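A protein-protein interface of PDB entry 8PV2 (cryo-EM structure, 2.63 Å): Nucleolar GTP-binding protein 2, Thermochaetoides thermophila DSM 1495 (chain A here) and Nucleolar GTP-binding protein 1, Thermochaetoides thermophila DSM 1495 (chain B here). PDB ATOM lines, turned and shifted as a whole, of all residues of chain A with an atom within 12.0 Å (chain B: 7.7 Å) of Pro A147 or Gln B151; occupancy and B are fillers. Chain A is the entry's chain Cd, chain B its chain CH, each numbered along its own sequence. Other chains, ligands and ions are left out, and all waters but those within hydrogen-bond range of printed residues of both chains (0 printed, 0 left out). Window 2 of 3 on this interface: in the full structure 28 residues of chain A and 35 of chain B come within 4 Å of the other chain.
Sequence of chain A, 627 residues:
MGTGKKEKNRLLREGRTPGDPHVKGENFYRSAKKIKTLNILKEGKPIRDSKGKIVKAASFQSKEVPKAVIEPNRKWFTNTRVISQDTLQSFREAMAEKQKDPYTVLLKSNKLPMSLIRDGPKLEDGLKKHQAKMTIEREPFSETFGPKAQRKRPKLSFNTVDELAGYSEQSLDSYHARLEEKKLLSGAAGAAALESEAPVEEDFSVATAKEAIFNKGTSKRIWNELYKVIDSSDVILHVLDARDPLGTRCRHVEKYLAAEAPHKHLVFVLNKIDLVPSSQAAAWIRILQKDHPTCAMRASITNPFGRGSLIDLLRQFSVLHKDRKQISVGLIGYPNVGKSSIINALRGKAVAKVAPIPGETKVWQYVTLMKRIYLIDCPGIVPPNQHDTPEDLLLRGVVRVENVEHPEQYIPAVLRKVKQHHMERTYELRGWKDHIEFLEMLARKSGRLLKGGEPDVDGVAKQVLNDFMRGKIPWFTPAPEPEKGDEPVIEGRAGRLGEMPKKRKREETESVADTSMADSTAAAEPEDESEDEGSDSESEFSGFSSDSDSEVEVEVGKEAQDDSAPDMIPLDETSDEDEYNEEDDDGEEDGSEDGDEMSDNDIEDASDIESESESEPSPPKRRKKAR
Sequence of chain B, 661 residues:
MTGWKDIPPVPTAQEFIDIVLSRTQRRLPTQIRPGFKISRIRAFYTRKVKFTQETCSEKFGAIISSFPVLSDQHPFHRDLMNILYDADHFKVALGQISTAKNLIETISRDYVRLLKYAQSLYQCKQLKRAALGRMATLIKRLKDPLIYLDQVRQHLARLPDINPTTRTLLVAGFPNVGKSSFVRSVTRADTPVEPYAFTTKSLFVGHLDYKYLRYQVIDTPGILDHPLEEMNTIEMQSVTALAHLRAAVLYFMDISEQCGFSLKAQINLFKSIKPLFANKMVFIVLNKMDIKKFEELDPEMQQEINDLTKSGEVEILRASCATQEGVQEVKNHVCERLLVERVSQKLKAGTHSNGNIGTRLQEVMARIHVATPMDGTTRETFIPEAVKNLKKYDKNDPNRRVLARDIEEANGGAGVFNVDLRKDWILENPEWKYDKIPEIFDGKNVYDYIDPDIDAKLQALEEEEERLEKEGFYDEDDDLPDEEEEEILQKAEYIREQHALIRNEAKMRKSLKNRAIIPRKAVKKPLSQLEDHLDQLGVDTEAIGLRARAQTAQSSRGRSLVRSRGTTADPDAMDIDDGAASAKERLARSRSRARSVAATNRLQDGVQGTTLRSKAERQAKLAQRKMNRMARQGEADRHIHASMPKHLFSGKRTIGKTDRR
The side-chain hydroxyl (OH) of Tyr B85 lies within hydrogen-bond range of a ring nitrogen (ND1) of His B155, 2.8 Å away.
The backbone NH (N) of Leu B156 is in hydrogen-bond range of the side-chain hydroxyl (OH) of Tyr B85 (3.3 Å).
Phe A141 touches Pro B145 (CE2 to CG, 3.6 Å).
CG of Tyr B148 touches CD1 of Phe A141, at 3.6 Å.
Phe A145 touches Tyr B85 (CZ to CE1, 3.5 Å).
CE1 of Tyr B148 touches CB of Phe A145, at 3.6 Å.
Gln B151 touches Phe A145 (O to CE2, 3.5 Å).
Val B152 touches Phe A145 (N to CE2, 3.9 Å).
His B155 touches Phe A145.
CD of Gln B151 touches CD of Pro A147, at 3.9 Å.
Pro A147 touches just one residue of chain B: Gln B151.
Gln B151 touches two residues of chain A.
No residue of chain A comes within 4 Å of Val B10.
Ile B147 touches none of the printed residues of chain A.
No residue of chain A comes within 4 Å of Asp B150.
Val B152 touches just one residue of chain A: Phe A145.
No residue of chain A comes within 4 Å of Gln B154.
Printed residues of chain A within 4 Å of Tyr B85: Phe A145.
Printed residues of chain A within 4 Å of Pro B145: Phe A141.
Leu B146 touches none of the printed residues of chain A.
Pro A140 touches none of the printed residues of chain B.
The nearest residue of chain B that does not touch Pro A147 is Ile B147 (6.3 Å).
The nearest residue of chain A that does not touch Gln B151 is Gly A146 (4.1 Å).
Printed residues of chain A that touch a printed residue of chain B: Phe A141, Phe A145 and Pro A147.
Hydrophobic or aromatic side chains of chain A that line the printed part of chain B: Phe A141, Phe A145 and Pro A147.
Among the printed residues, no Asp or Glu carboxylate lies within 4 Å of a Lys or Arg side-chain nitrogen of the other chain.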
ATOM      1  N   PRO A 140       0.301 -33.762  -9.763  1.00  0.00           N
ATOM      2  CA  PRO A 140      -0.265 -33.062 -10.921  1.00  0.00           C
ATOM      3  C   PRO A 140       0.273 -31.644 -11.048  1.00  0.00           C
ATOM      4  O   PRO A 140       0.854 -31.092 -10.112  1.00  0.00           O
ATOM      5  CB  PRO A 140      -1.774 -33.065 -10.644  1.00  0.00           C
ATOM      6  CG  PRO A 140      -1.931 -33.469  -9.234  1.00  0.00           C
ATOM      7  CD  PRO A 140      -0.736 -34.257  -8.847  1.00  0.00           C
ATOM      8  N   PHE A 141       0.089 -31.065 -12.237  1.00  0.00           N
ATOM      9  CA  PHE A 141       0.587 -29.717 -12.505  1.00  0.00           C
ATOM     10  C   PHE A 141      -0.124 -28.677 -11.649  1.00  0.00           C
ATOM     11  O   PHE A 141       0.469 -27.660 -11.273  1.00  0.00           O
ATOM     12  CB  PHE A 141       0.418 -29.373 -13.984  1.00  0.00           C
ATOM     13  CG  PHE A 141       1.505 -29.905 -14.863  1.00  0.00           C
ATOM     14  CD1 PHE A 141       2.808 -29.468 -14.716  1.00  0.00           C
ATOM     15  CD2 PHE A 141       1.222 -30.831 -15.851  1.00  0.00           C
ATOM     16  CE1 PHE A 141       3.808 -29.953 -15.525  1.00  0.00           C
ATOM     17  CE2 PHE A 141       2.220 -31.316 -16.665  1.00  0.00           C
ATOM     18  CZ  PHE A 141       3.514 -30.875 -16.503  1.00  0.00           C
ATOM     19  N   SER A 142      -1.398 -28.908 -11.339  1.00  0.00           N
ATOM     20  CA  SER A 142      -2.170 -27.943 -10.573  1.00  0.00           C
ATOM     21  C   SER A 142      -1.783 -27.916  -9.101  1.00  0.00           C
ATOM     22  O   SER A 142      -1.952 -26.879  -8.454  1.00  0.00           O
ATOM     23  CB  SER A 142      -3.659 -28.238 -10.716  1.00  0.00           C
ATOM     24  OG  SER A 142      -3.958 -29.550 -10.286  1.00  0.00           O
ATOM     25  N   GLU A 143      -1.283 -29.021  -8.555  1.00  0.00           N
ATOM     26  CA  GLU A 143      -0.846 -29.060  -7.168  1.00  0.00           C
ATOM     27  C   GLU A 143       0.575 -28.562  -6.969  1.00  0.00           C
ATOM     28  O   GLU A 143       0.978 -28.337  -5.826  1.00  0.00           O
ATOM     29  CB  GLU A 143      -0.944 -30.478  -6.609  1.00  0.00           C
ATOM     30  CG  GLU A 143      -2.351 -30.993  -6.434  1.00  0.00           C
ATOM     31  CD  GLU A 143      -2.376 -32.402  -5.890  1.00  0.00           C
ATOM     32  OE1 GLU A 143      -1.291 -33.004  -5.761  1.00  0.00           O
ATOM     33  OE2 GLU A 143      -3.476 -32.907  -5.584  1.00  0.00           O
ATOM     34  N   THR A 144       1.341 -28.386  -8.040  1.00  0.00           N
ATOM     35  CA  THR A 144       2.728 -27.960  -7.925  1.00  0.00           C
ATOM     36  C   THR A 144       2.858 -26.443  -7.904  1.00  0.00           C
ATOM     37  O   THR A 144       3.405 -25.876  -6.955  1.00  0.00           O
ATOM     38  CB  THR A 144       3.552 -28.544  -9.073  1.00  0.00           C
ATOM     39  OG1 THR A 144       3.553 -29.973  -8.981  1.00  0.00           O
ATOM     40  CG2 THR A 144       4.969 -28.039  -9.018  1.00  0.00           C
ATOM     41  N   PHE A 145       2.360 -25.776  -8.937  1.00  0.00           N
ATOM     42  CA  PHE A 145       2.429 -24.330  -9.026  1.00  0.00           C
ATOM     43  C   PHE A 145       1.095 -23.810  -9.536  1.00  0.00           C
ATOM     44  O   PHE A 145       0.480 -24.402 -10.424  1.00  0.00           O
ATOM     45  CB  PHE A 145       3.573 -23.884  -9.941  1.00  0.00           C
ATOM     46  CG  PHE A 145       3.971 -22.453  -9.761  1.00  0.00           C
ATOM     47  CD1 PHE A 145       4.746 -22.066  -8.682  1.00  0.00           C
ATOM     48  CD2 PHE A 145       3.577 -21.496 -10.673  1.00  0.00           C
ATOM     49  CE1 PHE A 145       5.112 -20.751  -8.518  1.00  0.00           C
ATOM     50  CE2 PHE A 145       3.942 -20.183 -10.513  1.00  0.00           C
ATOM     51  CZ  PHE A 145       4.710 -19.810  -9.435  1.00  0.00           C
ATOM     52  N   GLY A 146       0.654 -22.698  -8.964  1.00  0.00           N
ATOM     53  CA  GLY A 146      -0.619 -22.123  -9.313  1.00  0.00           C
ATOM     54  C   GLY A 146      -1.385 -21.670  -8.091  1.00  0.00           C
ATOM     55  O   GLY A 146      -0.902 -21.762  -6.958  1.00  0.00           O
ATOM     56  N   PRO A 147      -2.599 -21.156  -8.299  1.00  0.00           N
ATOM     57  CA  PRO A 147      -3.394 -20.667  -7.161  1.00  0.00           C
ATOM     58  C   PRO A 147      -3.846 -21.757  -6.205  1.00  0.00           C
ATOM     59  O   PRO A 147      -4.087 -21.463  -5.030  1.00  0.00           O
ATOM     60  CB  PRO A 147      -4.587 -19.982  -7.838  1.00  0.00           C
ATOM     61  CG  PRO A 147      -4.669 -20.601  -9.183  1.00  0.00           C
ATOM     62  CD  PRO A 147      -3.264 -20.910  -9.586  1.00  0.00           C
ATOM     63  N   LYS A 148      -3.961 -23.004  -6.660  1.00  0.00           N
ATOM     64  CA  LYS A 148      -4.393 -24.105  -5.808  1.00  0.00           C
ATOM     65  C   LYS A 148      -3.246 -25.050  -5.478  1.00  0.00           C
ATOM     66  O   LYS A 148      -3.486 -26.206  -5.120  1.00  0.00           O
ATOM     67  CB  LYS A 148      -5.535 -24.879  -6.467  1.00  0.00           C
ATOM     68  CG  LYS A 148      -6.685 -24.017  -6.963  1.00  0.00           C
ATOM     69  CD  LYS A 148      -7.213 -23.092  -5.884  1.00  0.00           C
ATOM     70  CE  LYS A 148      -8.156 -22.056  -6.471  1.00  0.00           C
ATOM     71  NZ  LYS A 148      -8.573 -21.052  -5.457  1.00  0.00           N
ATOM     72  N   ALA A 149      -2.007 -24.581  -5.600  1.00  0.00           N
ATOM     73  CA  ALA A 149      -0.847 -25.434  -5.392  1.00  0.00           C
ATOM     74  C   ALA A 149      -0.705 -25.815  -3.925  1.00  0.00           C
ATOM     75  O   ALA A 149      -0.951 -25.011  -3.022  1.00  0.00           O
ATOM     76  CB  ALA A 149       0.420 -24.730  -5.868  1.00  0.00           C
ATOM     77  N   GLN A 150      -0.301 -27.061  -3.693  1.00  0.00           N
ATOM     78  CA  GLN A 150      -0.120 -27.590  -2.352  1.00  0.00           C
ATOM     79  C   GLN A 150       1.307 -28.034  -2.082  1.00  0.00           C
ATOM     80  O   GLN A 150       1.555 -28.688  -1.064  1.00  0.00           O
ATOM     81  CB  GLN A 150      -1.076 -28.766  -2.113  1.00  0.00           C
ATOM     82  CG  GLN A 150      -2.535 -28.425  -2.321  1.00  0.00           C
ATOM     83  CD  GLN A 150      -3.016 -27.348  -1.381  1.00  0.00           C
ATOM     84  OE1 GLN A 150      -2.863 -27.456  -0.168  1.00  0.00           O
ATOM     85  NE2 GLN A 150      -3.596 -26.294  -1.936  1.00  0.00           N
ATOM     86  N   ARG A 151       2.247 -27.708  -2.962  1.00  0.00           N
ATOM     87  CA  ARG A 151       3.628 -28.129  -2.795  1.00  0.00           C
ATOM     88  C   ARG A 151       4.322 -27.275  -1.742  1.00  0.00           C
ATOM     89  O   ARG A 151       4.325 -26.045  -1.830  1.00  0.00           O
ATOM     90  CB  ARG A 151       4.356 -28.031  -4.132  1.00  0.00           C
ATOM     91  CG  ARG A 151       5.861 -28.085  -4.056  1.00  0.00           C
ATOM     92  CD  ARG A 151       6.441 -28.029  -5.452  1.00  0.00           C
ATOM     93  NE  ARG A 151       7.896 -27.979  -5.454  1.00  0.00           N
ATOM     94  CZ  ARG A 151       8.604 -26.864  -5.557  1.00  0.00           C
ATOM     95  NH1 ARG A 151       8.021 -25.684  -5.643  1.00  0.00           N
ATOM     96  NH2 ARG A 151       9.930 -26.940  -5.575  1.00  0.00           N
ATOM     97  N   LYS A 152       4.905 -27.929  -0.742  1.00  0.00           N
ATOM     98  CA  LYS A 152       5.608 -27.240   0.331  1.00  0.00           C
ATOM     99  C   LYS A 152       7.089 -27.566   0.392  1.00  0.00           C
ATOM    100  O   LYS A 152       7.910 -26.652   0.414  1.00  0.00           O
ATOM    101  CB  LYS A 152       4.963 -27.559   1.681  1.00  0.00           C
ATOM    102  CG  LYS A 152       3.640 -26.859   1.896  1.00  0.00           C
ATOM    103  CD  LYS A 152       3.857 -25.375   2.091  1.00  0.00           C
ATOM    104  CE  LYS A 152       2.573 -24.667   2.451  1.00  0.00           C
ATOM    105  NZ  LYS A 152       2.782 -23.199   2.542  1.00  0.00           N
ATOM    106  N   VAL B  10       1.028 -17.467 -22.530  1.00  0.00           N
ATOM    107  CA  VAL B  10       0.773 -18.863 -22.869  1.00  0.00           C
ATOM    108  C   VAL B  10      -0.736 -19.080 -22.804  1.00  0.00           C
ATOM    109  O   VAL B  10      -1.309 -19.020 -21.705  1.00  0.00           O
ATOM    110  CB  VAL B  10       1.513 -19.813 -21.919  1.00  0.00           C
ATOM    111  CG1 VAL B  10       1.239 -21.254 -22.288  1.00  0.00           C
ATOM    112  CG2 VAL B  10       3.000 -19.523 -21.918  1.00  0.00           C
ATOM    113  N   PHE B  67      11.096 -19.477 -22.872  1.00  0.00           N
ATOM    114  CA  PHE B  67      11.332 -19.901 -21.503  1.00  0.00           C
ATOM    115  C   PHE B  67      12.820 -20.149 -21.263  1.00  0.00           C
ATOM    116  O   PHE B  67      13.553 -20.500 -22.189  1.00  0.00           O
ATOM    117  CB  PHE B  67      10.536 -21.166 -21.198  1.00  0.00           C
ATOM    118  CG  PHE B  67       9.181 -20.901 -20.618  1.00  0.00           C
ATOM    119  CD1 PHE B  67       8.128 -20.521 -21.427  1.00  0.00           C
ATOM    120  CD2 PHE B  67       8.960 -21.039 -19.262  1.00  0.00           C
ATOM    121  CE1 PHE B  67       6.887 -20.277 -20.894  1.00  0.00           C
ATOM    122  CE2 PHE B  67       7.719 -20.795 -18.727  1.00  0.00           C
ATOM    123  CZ  PHE B  67       6.682 -20.414 -19.545  1.00  0.00           C
ATOM    124  N   TYR B  85       9.616 -23.597  -8.939  1.00  0.00           N
ATOM    125  CA  TYR B  85       8.725 -24.167  -9.937  1.00  0.00           C
ATOM    126  C   TYR B  85       8.827 -25.670 -10.142  1.00  0.00           C
ATOM    127  O   TYR B  85       8.130 -26.176 -11.028  1.00  0.00           O
ATOM    128  CB  TYR B  85       8.948 -23.501 -11.304  1.00  0.00           C
ATOM    129  CG  TYR B  85       9.000 -21.996 -11.285  1.00  0.00           C
ATOM    130  CD1 TYR B  85       7.902 -21.251 -10.892  1.00  0.00           C
ATOM    131  CD2 TYR B  85      10.145 -21.317 -11.684  1.00  0.00           C
ATOM    132  CE1 TYR B  85       7.946 -19.879 -10.881  1.00  0.00           C
ATOM    133  CE2 TYR B  85      10.197 -19.945 -11.675  1.00  0.00           C
ATOM    134  CZ  TYR B  85       9.093 -19.231 -11.273  1.00  0.00           C
ATOM    135  OH  TYR B  85       9.133 -17.859 -11.260  1.00  0.00           O
ATOM    136  N   PRO B 145      -0.242 -28.695 -18.725  1.00  0.00           N
ATOM    137  CA  PRO B 145       1.027 -27.974 -18.940  1.00  0.00           C
ATOM    138  C   PRO B 145       0.880 -26.518 -19.348  1.00  0.00           C
ATOM    139  O   PRO B 145       1.709 -25.700 -18.946  1.00  0.00           O
ATOM    140  CB  PRO B 145       1.700 -28.784 -20.053  1.00  0.00           C
ATOM    141  CG  PRO B 145       1.173 -30.112 -19.909  1.00  0.00           C
ATOM    142  CD  PRO B 145      -0.237 -29.958 -19.496  1.00  0.00           C
ATOM    143  N   LEU B 146      -0.146 -26.165 -20.122  1.00  0.00           N
ATOM    144  CA  LEU B 146      -0.293 -24.781 -20.559  1.00  0.00           C
ATOM    145  C   LEU B 146      -0.655 -23.867 -19.393  1.00  0.00           C
ATOM    146  O   LEU B 146      -0.132 -22.751 -19.276  1.00  0.00           O
ATOM    147  CB  LEU B 146      -1.337 -24.697 -21.669  1.00  0.00           C
ATOM    148  CG  LEU B 146      -0.916 -25.308 -23.006  1.00  0.00           C
ATOM    149  CD1 LEU B 146      -2.062 -25.286 -23.986  1.00  0.00           C
ATOM    150  CD2 LEU B 146       0.286 -24.593 -23.577  1.00  0.00           C
ATOM    151  N   ILE B 147      -1.541 -24.335 -18.511  1.00  0.00           N
ATOM    152  CA  ILE B 147      -1.908 -23.570 -17.321  1.00  0.00           C
ATOM    153  C   ILE B 147      -0.699 -23.398 -16.411  1.00  0.00           C
ATOM    154  O   ILE B 147      -0.414 -22.294 -15.914  1.00  0.00           O
ATOM    155  CB  ILE B 147      -3.075 -24.259 -16.594  1.00  0.00           C
ATOM    156  CG1 ILE B 147      -4.308 -24.290 -17.493  1.00  0.00           C
ATOM    157  CG2 ILE B 147      -3.389 -23.568 -15.286  1.00  0.00           C
ATOM    158  CD1 ILE B 147      -5.383 -25.217 -17.016  1.00  0.00           C
ATOM    159  N   TYR B 148       0.052 -24.489 -16.212  1.00  0.00           N
ATOM    160  CA  TYR B 148       1.247 -24.430 -15.381  1.00  0.00           C
ATOM    161  C   TYR B 148       2.278 -23.463 -15.955  1.00  0.00           C
ATOM    162  O   TYR B 148       2.860 -22.656 -15.218  1.00  0.00           O
ATOM    163  CB  TYR B 148       1.833 -25.834 -15.238  1.00  0.00           C
ATOM    164  CG  TYR B 148       3.218 -25.889 -14.646  1.00  0.00           C
ATOM    165  CD1 TYR B 148       3.405 -25.829 -13.278  1.00  0.00           C
ATOM    166  CD2 TYR B 148       4.339 -26.018 -15.457  1.00  0.00           C
ATOM    167  CE1 TYR B 148       4.663 -25.883 -12.732  1.00  0.00           C
ATOM    168  CE2 TYR B 148       5.599 -26.067 -14.920  1.00  0.00           C
ATOM    169  CZ  TYR B 148       5.756 -26.001 -13.555  1.00  0.00           C
ATOM    170  OH  TYR B 148       7.013 -26.055 -13.011  1.00  0.00           O
ATOM    171  N   LEU B 149       2.489 -23.506 -17.272  1.00  0.00           N
ATOM    172  CA  LEU B 149       3.483 -22.646 -17.898  1.00  0.00           C
ATOM    173  C   LEU B 149       3.063 -21.186 -17.887  1.00  0.00           C
ATOM    174  O   LEU B 149       3.924 -20.309 -17.790  1.00  0.00           O
ATOM    175  CB  LEU B 149       3.756 -23.104 -19.327  1.00  0.00           C
ATOM    176  CG  LEU B 149       4.664 -24.319 -19.509  1.00  0.00           C
ATOM    177  CD1 LEU B 149       4.750 -24.685 -20.976  1.00  0.00           C
ATOM    178  CD2 LEU B 149       6.041 -24.071 -18.932  1.00  0.00           C
ATOM    179  N   ASP B 150       1.764 -20.894 -17.980  1.00  0.00           N
ATOM    180  CA  ASP B 150       1.336 -19.501 -17.878  1.00  0.00           C
ATOM    181  C   ASP B 150       1.571 -18.945 -16.476  1.00  0.00           C
ATOM    182  O   ASP B 150       2.036 -17.802 -16.323  1.00  0.00           O
ATOM    183  CB  ASP B 150      -0.133 -19.368 -18.268  1.00  0.00           C
ATOM    184  CG  ASP B 150      -0.500 -17.953 -18.654  1.00  0.00           C
ATOM    185  OD1 ASP B 150       0.313 -17.289 -19.326  1.00  0.00           O
ATOM    186  OD2 ASP B 150      -1.592 -17.492 -18.271  1.00  0.00           O
ATOM    187  N   GLN B 151       1.268 -19.742 -15.443  1.00  0.00           N
ATOM    188  CA  GLN B 151       1.548 -19.304 -14.075  1.00  0.00           C
ATOM    189  C   GLN B 151       3.043 -19.077 -13.860  1.00  0.00           C
ATOM    190  O   GLN B 151       3.455 -18.064 -13.265  1.00  0.00           O
ATOM    191  CB  GLN B 151       1.026 -20.338 -13.079  1.00  0.00           C
ATOM    192  CG  GLN B 151      -0.466 -20.576 -13.123  1.00  0.00           C
ATOM    193  CD  GLN B 151      -1.264 -19.397 -12.631  1.00  0.00           C
ATOM    194  OE1 GLN B 151      -0.795 -18.613 -11.807  1.00  0.00           O
ATOM    195  NE2 GLN B 151      -2.484 -19.263 -13.131  1.00  0.00           N
ATOM    196  N   VAL B 152       3.865 -20.001 -14.365  1.00  0.00           N
ATOM    197  CA  VAL B 152       5.316 -19.880 -14.257  1.00  0.00           C
ATOM    198  C   VAL B 152       5.809 -18.647 -15.004  1.00  0.00           C
ATOM    199  O   VAL B 152       6.710 -17.944 -14.536  1.00  0.00           O
ATOM    200  CB  VAL B 152       5.984 -21.172 -14.764  1.00  0.00           C
ATOM    201  CG1 VAL B 152       7.471 -20.987 -14.968  1.00  0.00           C
ATOM    202  CG2 VAL B 152       5.749 -22.292 -13.790  1.00  0.00           C
ATOM    203  N   ARG B 153       5.207 -18.351 -16.158  1.00  0.00           N
ATOM    204  CA  ARG B 153       5.594 -17.183 -16.940  1.00  0.00           C
ATOM    205  C   ARG B 153       5.338 -15.889 -16.183  1.00  0.00           C
ATOM    206  O   ARG B 153       6.187 -14.991 -16.174  1.00  0.00           O
ATOM    207  CB  ARG B 153       4.834 -17.173 -18.265  1.00  0.00           C
ATOM    208  CG  ARG B 153       4.990 -15.889 -19.042  1.00  0.00           C
ATOM    209  CD  ARG B 153       3.896 -15.705 -20.058  1.00  0.00           C
ATOM    210  NE  ARG B 153       2.632 -15.249 -19.493  1.00  0.00           N
ATOM    211  CZ  ARG B 153       2.313 -13.976 -19.303  1.00  0.00           C
ATOM    212  NH1 ARG B 153       3.182 -13.006 -19.529  1.00  0.00           N
ATOM    213  NH2 ARG B 153       1.093 -13.668 -18.876  1.00  0.00           N
ATOM    214  N   GLN B 154       4.172 -15.772 -15.547  1.00  0.00           N
ATOM    215  CA  GLN B 154       3.871 -14.547 -14.809  1.00  0.00           C
ATOM    216  C   GLN B 154       4.798 -14.372 -13.608  1.00  0.00           C
ATOM    217  O   GLN B 154       5.301 -13.264 -13.349  1.00  0.00           O
ATOM    218  CB  GLN B 154       2.409 -14.550 -14.379  1.00  0.00           C
ATOM    219  CG  GLN B 154       1.456 -14.521 -15.551  1.00  0.00           C
ATOM    220  CD  GLN B 154       0.024 -14.330 -15.131  1.00  0.00           C
ATOM    221  OE1 GLN B 154      -0.260 -14.002 -13.983  1.00  0.00           O
ATOM    222  NE2 GLN B 154      -0.894 -14.535 -16.063  1.00  0.00           N
ATOM    223  N   HIS B 155       5.072 -15.463 -12.886  1.00  0.00           N
ATOM    224  CA  HIS B 155       5.986 -15.366 -11.750  1.00  0.00           C
ATOM    225  C   HIS B 155       7.408 -15.018 -12.197  1.00  0.00           C
ATOM    226  O   HIS B 155       8.080 -14.184 -11.573  1.00  0.00           O
ATOM    227  CB  HIS B 155       5.963 -16.673 -10.962  1.00  0.00           C
ATOM    228  CG  HIS B 155       6.428 -16.533  -9.549  1.00  0.00           C
ATOM    229  ND1 HIS B 155       7.737 -16.732  -9.174  1.00  0.00           N
ATOM    230  CD2 HIS B 155       5.755 -16.218  -8.420  1.00  0.00           C
ATOM    231  CE1 HIS B 155       7.851 -16.543  -7.873  1.00  0.00           C
ATOM    232  NE2 HIS B 155       6.663 -16.232  -7.391  1.00  0.00           N
ATOM    233  N   LEU B 156       7.871 -15.632 -13.292  1.00  0.00           N
ATOM    234  CA  LEU B 156       9.191 -15.338 -13.839  1.00  0.00           C
ATOM    235  C   LEU B 156       9.299 -13.898 -14.303  1.00  0.00           C
ATOM    236  O   LEU B 156      10.355 -13.277 -14.156  1.00  0.00           O
ATOM    237  CB  LEU B 156       9.502 -16.272 -15.006  1.00  0.00           C
ATOM    238  CG  LEU B 156      10.151 -17.626 -14.752  1.00  0.00           C
ATOM    239  CD1 LEU B 156      10.061 -18.470 -15.999  1.00  0.00           C
ATOM    240  CD2 LEU B 156      11.594 -17.452 -14.348  1.00  0.00           C
ATOM    241  N   ALA B 157       8.226 -13.361 -14.888  1.00  0.00           N
ATOM    242  CA  ALA B 157       8.209 -11.959 -15.273  1.00  0.00           C
ATOM    243  C   ALA B 157       8.305 -11.036 -14.075  1.00  0.00           C
ATOM    244  O   ALA B 157       8.914  -9.968 -14.181  1.00  0.00           O
ATOM    245  CB  ALA B 157       6.944 -11.645 -16.064  1.00  0.00           C
ATOM    246  N   ARG B 158       7.725 -11.418 -12.939  1.00  0.00           N
ATOM    247  CA  ARG B 158       7.807 -10.581 -11.748  1.00  0.00           C
ATOM    248  C   ARG B 158       9.000 -10.901 -10.847  1.00  0.00           C
ATOM    249  O   ARG B 158       9.109 -10.315  -9.768  1.00  0.00           O
ATOM    250  CB  ARG B 158       6.508 -10.676 -10.953  1.00  0.00           C
ATOM    251  CG  ARG B 158       5.286 -10.300 -11.750  1.00  0.00           C
ATOM    252  CD  ARG B 158       4.112 -10.032 -10.844  1.00  0.00           C
ATOM    253  NE  ARG B 158       3.936 -11.101  -9.872  1.00  0.00           N
ATOM    254  CZ  ARG B 158       3.211 -12.192 -10.075  1.00  0.00           C
ATOM    255  NH1 ARG B 158       2.581 -12.399 -11.218  1.00  0.00           N
ATOM    256  NH2 ARG B 158       3.123 -13.100  -9.111  1.00  0.00           N
